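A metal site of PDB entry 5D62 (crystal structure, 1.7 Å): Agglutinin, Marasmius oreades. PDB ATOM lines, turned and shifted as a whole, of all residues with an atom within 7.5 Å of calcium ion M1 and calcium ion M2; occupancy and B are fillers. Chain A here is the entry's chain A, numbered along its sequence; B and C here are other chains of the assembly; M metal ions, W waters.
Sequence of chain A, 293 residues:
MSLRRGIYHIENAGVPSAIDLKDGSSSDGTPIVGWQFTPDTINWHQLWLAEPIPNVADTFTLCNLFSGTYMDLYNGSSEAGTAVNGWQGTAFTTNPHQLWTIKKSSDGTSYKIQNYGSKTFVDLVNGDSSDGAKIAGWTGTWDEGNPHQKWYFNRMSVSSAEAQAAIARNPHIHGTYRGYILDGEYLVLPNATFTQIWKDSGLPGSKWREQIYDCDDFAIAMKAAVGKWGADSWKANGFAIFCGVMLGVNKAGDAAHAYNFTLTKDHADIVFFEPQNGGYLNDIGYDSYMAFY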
ATOM      1  N   TRP A 208      27.834   1.711 -33.766  1.00  0.00           N
ATOM      2  CA  TRP A 208      27.272   0.412 -33.724  1.00  0.00           C
ATOM      3  C   TRP A 208      28.448  -0.608 -33.622  1.00  0.00           C
ATOM      4  O   TRP A 208      29.395  -0.576 -34.438  1.00  0.00           O
ATOM      5  CB  TRP A 208      26.437   0.135 -34.962  1.00  0.00           C
ATOM      6  CG  TRP A 208      25.743  -1.207 -34.975  1.00  0.00           C
ATOM      7  CD1 TRP A 208      24.443  -1.474 -34.536  1.00  0.00           C
ATOM      8  CD2 TRP A 208      26.284  -2.484 -35.314  1.00  0.00           C
ATOM      9  NE1 TRP A 208      24.169  -2.806 -34.644  1.00  0.00           N
ATOM     10  CE2 TRP A 208      25.264  -3.445 -35.123  1.00  0.00           C
ATOM     11  CE3 TRP A 208      27.513  -2.912 -35.804  1.00  0.00           C
ATOM     12  CZ2 TRP A 208      25.440  -4.804 -35.411  1.00  0.00           C
ATOM     13  CZ3 TRP A 208      27.689  -4.257 -36.093  1.00  0.00           C
ATOM     14  CH2 TRP A 208      26.669  -5.175 -35.903  1.00  0.00           C
ATOM     15  N   ARG A 209      28.287  -1.523 -32.698  1.00  0.00           N
ATOM     16  CA  ARG A 209      29.271  -2.602 -32.449  1.00  0.00           C
ATOM     17  C   ARG A 209      28.478  -3.871 -32.117  1.00  0.00           C
ATOM     18  O   ARG A 209      27.566  -3.846 -31.273  1.00  0.00           O
ATOM     19  CB  ARG A 209      30.221  -2.251 -31.348  1.00  0.00           C
ATOM     20  CG  ARG A 209      31.115  -1.016 -31.590  1.00  0.00           C
ATOM     21  CD  ARG A 209      31.874  -0.497 -30.347  1.00  0.00           C
ATOM     22  NE  ARG A 209      32.740  -1.554 -29.820  1.00  0.00           N
ATOM     23  CZ  ARG A 209      33.292  -1.602 -28.617  1.00  0.00           C
ATOM     24  NH1 ARG A 209      33.224  -0.554 -27.794  1.00  0.00           N
ATOM     25  NH2 ARG A 209      33.936  -2.699 -28.271  1.00  0.00           N
ATOM     26  N   GLU A 210      28.852  -4.966 -32.795  1.00  0.00           N
ATOM     27  CA  GLU A 210      28.137  -6.254 -32.649  1.00  0.00           C
ATOM     28  C   GLU A 210      28.040  -6.709 -31.172  1.00  0.00           C
ATOM     29  O   GLU A 210      29.065  -6.862 -30.400  1.00  0.00           O
ATOM     30  CB  GLU A 210      28.854  -7.334 -33.547  1.00  0.00           C
ATOM     31  CG  GLU A 210      28.081  -8.629 -33.675  1.00  0.00           C
ATOM     32  CD  GLU A 210      28.765  -9.626 -34.615  1.00  0.00           C
ATOM     33  OE1 GLU A 210      29.775  -9.300 -35.257  1.00  0.00           O
ATOM     34  OE2 GLU A 210      28.287 -10.751 -34.700  1.00  0.00           O
ATOM     35  N   GLN A 211      26.802  -6.906 -30.750  1.00  0.00           N
ATOM     36  CA  GLN A 211      26.367  -7.173 -29.409  1.00  0.00           C
ATOM     37  C   GLN A 211      26.727  -6.183 -28.295  1.00  0.00           C
ATOM     38  O   GLN A 211      25.912  -5.888 -27.433  1.00  0.00           O
ATOM     39  CB  GLN A 211      26.780  -8.592 -28.960  1.00  0.00           C
ATOM     40  CG  GLN A 211      26.157  -9.688 -29.851  1.00  0.00           C
ATOM     41  CD  GLN A 211      26.291 -11.093 -29.207  1.00  0.00           C
ATOM     42  OE1 GLN A 211      25.994 -11.287 -28.028  1.00  0.00           O
ATOM     43  NE2 GLN A 211      26.766 -12.057 -30.017  1.00  0.00           N
ATOM     44  N   ILE A 212      27.947  -5.642 -28.297  1.00  0.00           N
ATOM     45  CA  ILE A 212      28.415  -4.799 -27.120  1.00  0.00           C
ATOM     46  C   ILE A 212      27.822  -3.391 -27.192  1.00  0.00           C
ATOM     47  O   ILE A 212      27.793  -2.727 -26.152  1.00  0.00           O
ATOM     48  CB  ILE A 212      29.972  -4.791 -27.142  1.00  0.00           C
ATOM     49  CG1 ILE A 212      30.623  -4.270 -25.825  1.00  0.00           C
ATOM     50  CG2 ILE A 212      30.502  -4.060 -28.326  1.00  0.00           C
ATOM     51  CD1 ILE A 212      30.259  -5.128 -24.604  1.00  0.00           C
ATOM     52  N   TYR A 213      27.478  -2.898 -28.383  1.00  0.00           N
ATOM     53  CA  TYR A 213      26.666  -1.660 -28.457  1.00  0.00           C
ATOM     54  C   TYR A 213      25.894  -1.642 -29.769  1.00  0.00           C
ATOM     55  O   TYR A 213      26.217  -0.969 -30.747  1.00  0.00           O
ATOM     56  CB  TYR A 213      27.552  -0.434 -28.255  1.00  0.00           C
ATOM     57  CG  TYR A 213      26.803   0.644 -27.459  1.00  0.00           C
ATOM     58  CD1 TYR A 213      26.669   0.560 -26.095  1.00  0.00           C
ATOM     59  CD2 TYR A 213      26.282   1.760 -28.104  1.00  0.00           C
ATOM     60  CE1 TYR A 213      25.973   1.508 -25.385  1.00  0.00           C
ATOM     61  CE2 TYR A 213      25.576   2.728 -27.438  1.00  0.00           C
ATOM     62  CZ  TYR A 213      25.402   2.610 -26.063  1.00  0.00           C
ATOM     63  OH  TYR A 213      24.708   3.581 -25.280  1.00  0.00           O
ATOM     64  N   ASP A 214      24.864  -2.466 -29.761  1.00  0.00           N
ATOM     65  CA  ASP A 214      24.091  -2.700 -30.953  1.00  0.00           C
ATOM     66  C   ASP A 214      22.701  -2.108 -30.685  1.00  0.00           C
ATOM     67  O   ASP A 214      22.502  -1.257 -29.809  1.00  0.00           O
ATOM     68  CB  ASP A 214      24.088  -4.212 -31.419  1.00  0.00           C
ATOM     69  CG  ASP A 214      23.437  -5.168 -30.468  1.00  0.00           C
ATOM     70  OD1 ASP A 214      23.392  -4.873 -29.226  1.00  0.00           O
ATOM     71  OD2 ASP A 214      23.017  -6.324 -30.910  1.00  0.00           O
ATOM     72  N   CYS A 215      21.725  -2.522 -31.471  1.00  0.00           N
ATOM     73  CA  CYS A 215      20.480  -1.743 -31.584  1.00  0.00           C
ATOM     74  C   CYS A 215      19.829  -1.697 -30.206  1.00  0.00           C
ATOM     75  O   CYS A 215      19.273  -0.666 -29.833  1.00  0.00           O
ATOM     76  CB  CYS A 215      19.512  -2.320 -32.673  1.00  0.00           C
ATOM     77  SG  CYS A 215      19.146  -4.102 -32.452  1.00  0.00           S
ATOM     78  N   ASP A 216      19.811  -2.816 -29.486  1.00  0.00           N
ATOM     79  CA  ASP A 216      19.185  -2.844 -28.202  1.00  0.00           C
ATOM     80  C   ASP A 216      19.825  -1.851 -27.232  1.00  0.00           C
ATOM     81  O   ASP A 216      19.133  -1.204 -26.398  1.00  0.00           O
ATOM     82  CB  ASP A 216      19.095  -4.199 -27.568  1.00  0.00           C
ATOM     83  CG  ASP A 216      20.398  -4.978 -27.698  1.00  0.00           C
ATOM     84  OD1 ASP A 216      20.567  -5.664 -28.742  1.00  0.00           O
ATOM     85  OD2 ASP A 216      21.194  -4.920 -26.754  1.00  0.00           O
ATOM     86  N   ASP A 217      21.151  -1.666 -27.300  1.00  0.00           N
ATOM     87  CA  ASP A 217      21.808  -0.676 -26.397  1.00  0.00           C
ATOM     88  C   ASP A 217      21.404   0.781 -26.741  1.00  0.00           C
ATOM     89  O   ASP A 217      21.227   1.598 -25.807  1.00  0.00           O
ATOM     90  CB  ASP A 217      23.345  -0.805 -26.535  1.00  0.00           C
ATOM     91  CG  ASP A 217      23.805  -2.217 -26.126  1.00  0.00           C
ATOM     92  OD1 ASP A 217      23.873  -2.427 -24.943  1.00  0.00           O
ATOM     93  OD2 ASP A 217      24.014  -3.139 -26.987  1.00  0.00           O
ATOM     94  N   PHE A 218      21.340   1.128 -28.051  1.00  0.00           N
ATOM     95  CA  PHE A 218      20.894   2.442 -28.454  1.00  0.00           C
ATOM     96  C   PHE A 218      19.497   2.721 -27.962  1.00  0.00           C
ATOM     97  O   PHE A 218      19.190   3.776 -27.452  1.00  0.00           O
ATOM     98  CB  PHE A 218      20.932   2.599 -29.980  1.00  0.00           C
ATOM     99  CG  PHE A 218      22.277   2.841 -30.561  1.00  0.00           C
ATOM    100  CD1 PHE A 218      23.175   1.741 -30.841  1.00  0.00           C
ATOM    101  CD2 PHE A 218      22.613   4.065 -31.044  1.00  0.00           C
ATOM    102  CE1 PHE A 218      24.395   1.989 -31.477  1.00  0.00           C
ATOM    103  CE2 PHE A 218      23.876   4.344 -31.565  1.00  0.00           C
ATOM    104  CZ  PHE A 218      24.759   3.316 -31.790  1.00  0.00           C
ATOM    105  N   ALA A 258      15.729  -3.295 -32.573  1.00  0.00           N
ATOM    106  CA  ALA A 258      15.289  -2.582 -31.364  1.00  0.00           C
ATOM    107  C   ALA A 258      15.332  -1.070 -31.684  1.00  0.00           C
ATOM    108  O   ALA A 258      16.272  -0.588 -32.338  1.00  0.00           O
ATOM    109  CB  ALA A 258      16.190  -2.901 -30.205  1.00  0.00           C
ATOM    110  N   ILE B 181      15.168 -11.782 -24.902  1.00  0.00           N
ATOM    111  CA  ILE B 181      16.603 -11.941 -25.097  1.00  0.00           C
ATOM    112  C   ILE B 181      17.081 -10.922 -26.085  1.00  0.00           C
ATOM    113  O   ILE B 181      16.584 -10.836 -27.192  1.00  0.00           O
ATOM    114  CB  ILE B 181      16.940 -13.362 -25.549  1.00  0.00           C
ATOM    115  CG1 ILE B 181      16.593 -14.306 -24.393  1.00  0.00           C
ATOM    116  CG2 ILE B 181      18.422 -13.491 -25.949  1.00  0.00           C
ATOM    117  CD1 ILE B 181      16.791 -15.787 -24.735  1.00  0.00           C
ATOM    118  N   LEU B 182      18.167 -10.195 -25.724  1.00  0.00           N
ATOM    119  CA  LEU B 182      18.653  -9.130 -26.577  1.00  0.00           C
ATOM    120  C   LEU B 182      19.957  -9.394 -27.300  1.00  0.00           C
ATOM    121  O   LEU B 182      20.291  -8.758 -28.347  1.00  0.00           O
ATOM    122  CB  LEU B 182      18.755  -7.917 -25.652  1.00  0.00           C
ATOM    123  CG  LEU B 182      17.515  -7.363 -24.930  1.00  0.00           C
ATOM    124  CD1 LEU B 182      17.863  -6.201 -24.021  1.00  0.00           C
ATOM    125  CD2 LEU B 182      16.565  -6.885 -25.961  1.00  0.00           C
ATOM    126  N   ASP B 183      20.781 -10.266 -26.727  1.00  0.00           N
ATOM    127  CA  ASP B 183      22.096 -10.569 -27.322  1.00  0.00           C
ATOM    128  C   ASP B 183      22.367 -12.123 -27.218  1.00  0.00           C
ATOM    129  O   ASP B 183      21.464 -12.888 -26.836  1.00  0.00           O
ATOM    130  CB  ASP B 183      23.161  -9.782 -26.575  1.00  0.00           C
ATOM    131  CG  ASP B 183      23.064  -8.253 -26.808  1.00  0.00           C
ATOM    132  OD1 ASP B 183      23.147  -7.802 -27.958  1.00  0.00           O
ATOM    133  OD2 ASP B 183      22.972  -7.490 -25.809  1.00  0.00           O
ATOM    134  N   GLY B 184      23.574 -12.560 -27.517  1.00  0.00           N
ATOM    135  CA  GLY B 184      23.938 -14.000 -27.630  1.00  0.00           C
ATOM    136  C   GLY B 184      24.896 -14.536 -26.626  1.00  0.00           C
ATOM    137  O   GLY B 184      24.828 -15.735 -26.270  1.00  0.00           O
ATOM    138  N   TYR B 186      27.320 -13.331 -23.036  1.00  0.00           N
ATOM    139  CA  TYR B 186      27.425 -12.285 -22.013  1.00  0.00           C
ATOM    140  C   TYR B 186      28.538 -12.489 -21.019  1.00  0.00           C
ATOM    141  O   TYR B 186      28.624 -13.504 -20.337  1.00  0.00           O
ATOM    142  CB  TYR B 186      26.128 -12.281 -21.229  1.00  0.00           C
ATOM    143  CG  TYR B 186      24.838 -11.992 -21.971  1.00  0.00           C
ATOM    144  CD1 TYR B 186      24.367 -10.666 -22.143  1.00  0.00           C
ATOM    145  CD2 TYR B 186      24.056 -13.008 -22.482  1.00  0.00           C
ATOM    146  CE1 TYR B 186      23.179 -10.396 -22.797  1.00  0.00           C
ATOM    147  CE2 TYR B 186      22.823 -12.772 -23.105  1.00  0.00           C
ATOM    148  CZ  TYR B 186      22.343 -11.493 -23.216  1.00  0.00           C
ATOM    149  OH  TYR B 186      21.165 -11.216 -23.826  1.00  0.00           O
ATOM    150  N   LYS B 223      20.616  -0.773 -16.124  1.00  0.00           N
ATOM    151  CA  LYS B 223      20.896  -1.549 -17.311  1.00  0.00           C
ATOM    152  C   LYS B 223      21.644  -0.688 -18.379  1.00  0.00           C
ATOM    153  O   LYS B 223      22.586  -1.155 -19.027  1.00  0.00           O
ATOM    154  CB  LYS B 223      19.649  -2.135 -17.978  1.00  0.00           C
ATOM    155  CG  LYS B 223      20.027  -3.011 -19.199  1.00  0.00           C
ATOM    156  CD  LYS B 223      18.986  -4.112 -19.538  1.00  0.00           C
ATOM    157  CE  LYS B 223      19.417  -4.981 -20.765  1.00  0.00           C
ATOM    158  NZ  LYS B 223      20.873  -5.460 -20.760  1.00  0.00           N
ATOM    159  N   GLY B 227      25.446  -1.267 -19.963  1.00  0.00           N
ATOM    160  CA  GLY B 227      25.683  -1.250 -21.412  1.00  0.00           C
ATOM    161  C   GLY B 227      26.746  -0.210 -21.821  1.00  0.00           C
ATOM    162  O   GLY B 227      27.622  -0.518 -22.636  1.00  0.00           O
ATOM    163  N   PHE B 239      30.141  -9.754 -28.100  1.00  0.00           N
ATOM    164  CA  PHE B 239      29.618 -10.158 -26.840  1.00  0.00           C
ATOM    165  C   PHE B 239      28.933  -8.928 -26.176  1.00  0.00           C
ATOM    166  O   PHE B 239      29.164  -7.787 -26.591  1.00  0.00           O
ATOM    167  CB  PHE B 239      30.734 -10.660 -25.910  1.00  0.00           C
ATOM    168  CG  PHE B 239      31.680  -9.548 -25.462  1.00  0.00           C
ATOM    169  CD1 PHE B 239      32.612  -9.023 -26.337  1.00  0.00           C
ATOM    170  CD2 PHE B 239      31.625  -9.040 -24.186  1.00  0.00           C
ATOM    171  CE1 PHE B 239      33.451  -7.934 -25.958  1.00  0.00           C
ATOM    172  CE2 PHE B 239      32.489  -7.979 -23.790  1.00  0.00           C
ATOM    173  CZ  PHE B 239      33.349  -7.447 -24.694  1.00  0.00           C
ATOM    174  N   ALA B 240      28.142  -9.202 -25.147  1.00  0.00           N
ATOM    175  CA  ALA B 240      27.514  -8.194 -24.306  1.00  0.00           C
ATOM    176  C   ALA B 240      27.902  -8.369 -22.843  1.00  0.00           C
ATOM    177  O   ALA B 240      28.578  -9.345 -22.481  1.00  0.00           O
ATOM    178  CB  ALA B 240      26.012  -8.215 -24.465  1.00  0.00           C
ATOM    179  N   ILE B 241      27.474  -7.467 -21.956  1.00  0.00           N
ATOM    180  CA  ILE B 241      27.659  -7.621 -20.527  1.00  0.00           C
ATOM    181  C   ILE B 241      26.319  -8.030 -19.856  1.00  0.00           C
ATOM    182  O   ILE B 241      25.288  -7.412 -20.167  1.00  0.00           O
ATOM    183  CB  ILE B 241      28.008  -6.325 -19.901  1.00  0.00           C
ATOM    184  CG1 ILE B 241      29.166  -5.636 -20.720  1.00  0.00           C
ATOM    185  CG2 ILE B 241      28.419  -6.479 -18.442  1.00  0.00           C
ATOM    186  CD1 ILE B 241      30.446  -6.411 -20.959  1.00  0.00           C
ATOM    187  N   TYR B 293      17.125  -8.780 -21.093  1.00  0.00           N
ATOM    188  CA  TYR B 293      18.557  -8.932 -20.750  1.00  0.00           C
ATOM    189  C   TYR B 293      19.276  -9.273 -22.051  1.00  0.00           C
ATOM    190  O   TYR B 293      20.429  -8.942 -22.210  1.00  0.00           O
ATOM    191  CB  TYR B 293      18.762 -10.044 -19.713  1.00  0.00           C
ATOM    192  CG  TYR B 293      18.136 -11.394 -20.039  1.00  0.00           C
ATOM    193  CD1 TYR B 293      16.790 -11.706 -19.704  1.00  0.00           C
ATOM    194  CD2 TYR B 293      18.907 -12.368 -20.646  1.00  0.00           C
ATOM    195  CE1 TYR B 293      16.258 -12.957 -19.997  1.00  0.00           C
ATOM    196  CE2 TYR B 293      18.353 -13.634 -20.965  1.00  0.00           C
ATOM    197  CZ  TYR B 293      17.063 -13.924 -20.595  1.00  0.00           C
ATOM    198  OH  TYR B 293      16.540 -15.224 -20.895  1.00  0.00           O
ATOM    199  OXT TYR B 293      18.676  -9.841 -23.012  1.00  0.00           O
ATOM    200  N   ASP C   4      21.758  -4.225 -36.983  1.00  0.00           N
ATOM    201  CA  ASP C   4      21.006  -5.106 -36.175  1.00  0.00           C
ATOM    202  C   ASP C   4      20.791  -4.691 -34.680  1.00  0.00           C
ATOM    203  O   ASP C   4      21.778  -4.379 -33.993  1.00  0.00           O
ATOM    204  CB  ASP C   4      21.774  -6.439 -36.183  1.00  0.00           C
ATOM    205  CG  ASP C   4      20.917  -7.587 -35.861  1.00  0.00           C
ATOM    206  OD1 ASP C   4      19.704  -7.367 -35.702  1.00  0.00           O
ATOM    207  OD2 ASP C   4      21.472  -8.705 -35.787  1.00  0.00           O
ATOM    208  C1  CF0 C   5      19.443  -4.648 -34.035  1.00  0.00           C
HETATM  209 CA    CA M   1      21.548  -7.539 -29.683  1.00  0.00          CA
HETATM  210 CA    CA M   2      23.570  -5.472 -26.989  1.00  0.00          CA
HETATM  211  O   HOH W   1      22.349  -9.560 -30.832  1.00  0.00           O
HETATM  212  O   HOH W   2      23.953  -5.024 -24.716  1.00  0.00           O
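OXT of Tyr 293 of chain B lies within hydrogen-bond range of N of Leu 182 of chain B, 2.8 Å away. N of Asp 214 is in hydrogen-bond range of O of Arg 209 (3.4 Å). The side-chain hydroxyl of Tyr 186 of chain B is in hydrogen-bond range of the backbone NH of Asp 183 of chain B, at 3.1 Å. N of Gly 184 of chain B is in hydrogen-bond range of OE1 of Gln 211.
Within 4 Å of calcium ion M2: Gln 211, Asp 214, Asp 216, Asp 217 and Asp 183 of chain B.
Calcium ion M1 is bound by O of Leu 182 of chain B, OD2 of Asp 214, OD1 of Asp 216, OD1 of Asp 183 of chain B and water W1. Calcium ion M1 has five donor atoms within binding distance.
Within 4 Å of calcium ion M1: Asp 214, Asp 216, Leu 182 of chain B and Asp 183 of chain B.
Calcium ion M2 is bound by the side-chain carboxylate (OD1) of Asp 214 (2.3 Å), water W2 (2.3 Å), the side-chain carboxylate (OD2) of Asp 217 (2.4 Å), the side-chain carboxylate (OD2) of Asp 183 of chain B (2.4 Å), the backbone carbonyl oxygen (O) of Gln 211 (2.4 Å), the side-chain carboxylate (OD2) of Asp 216 (2.5 Å) and the side-chain carboxylate (OD1) of Asp 183 of chain B (2.6 Å). Calcium ion M2 has seven donor atoms within binding distance.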
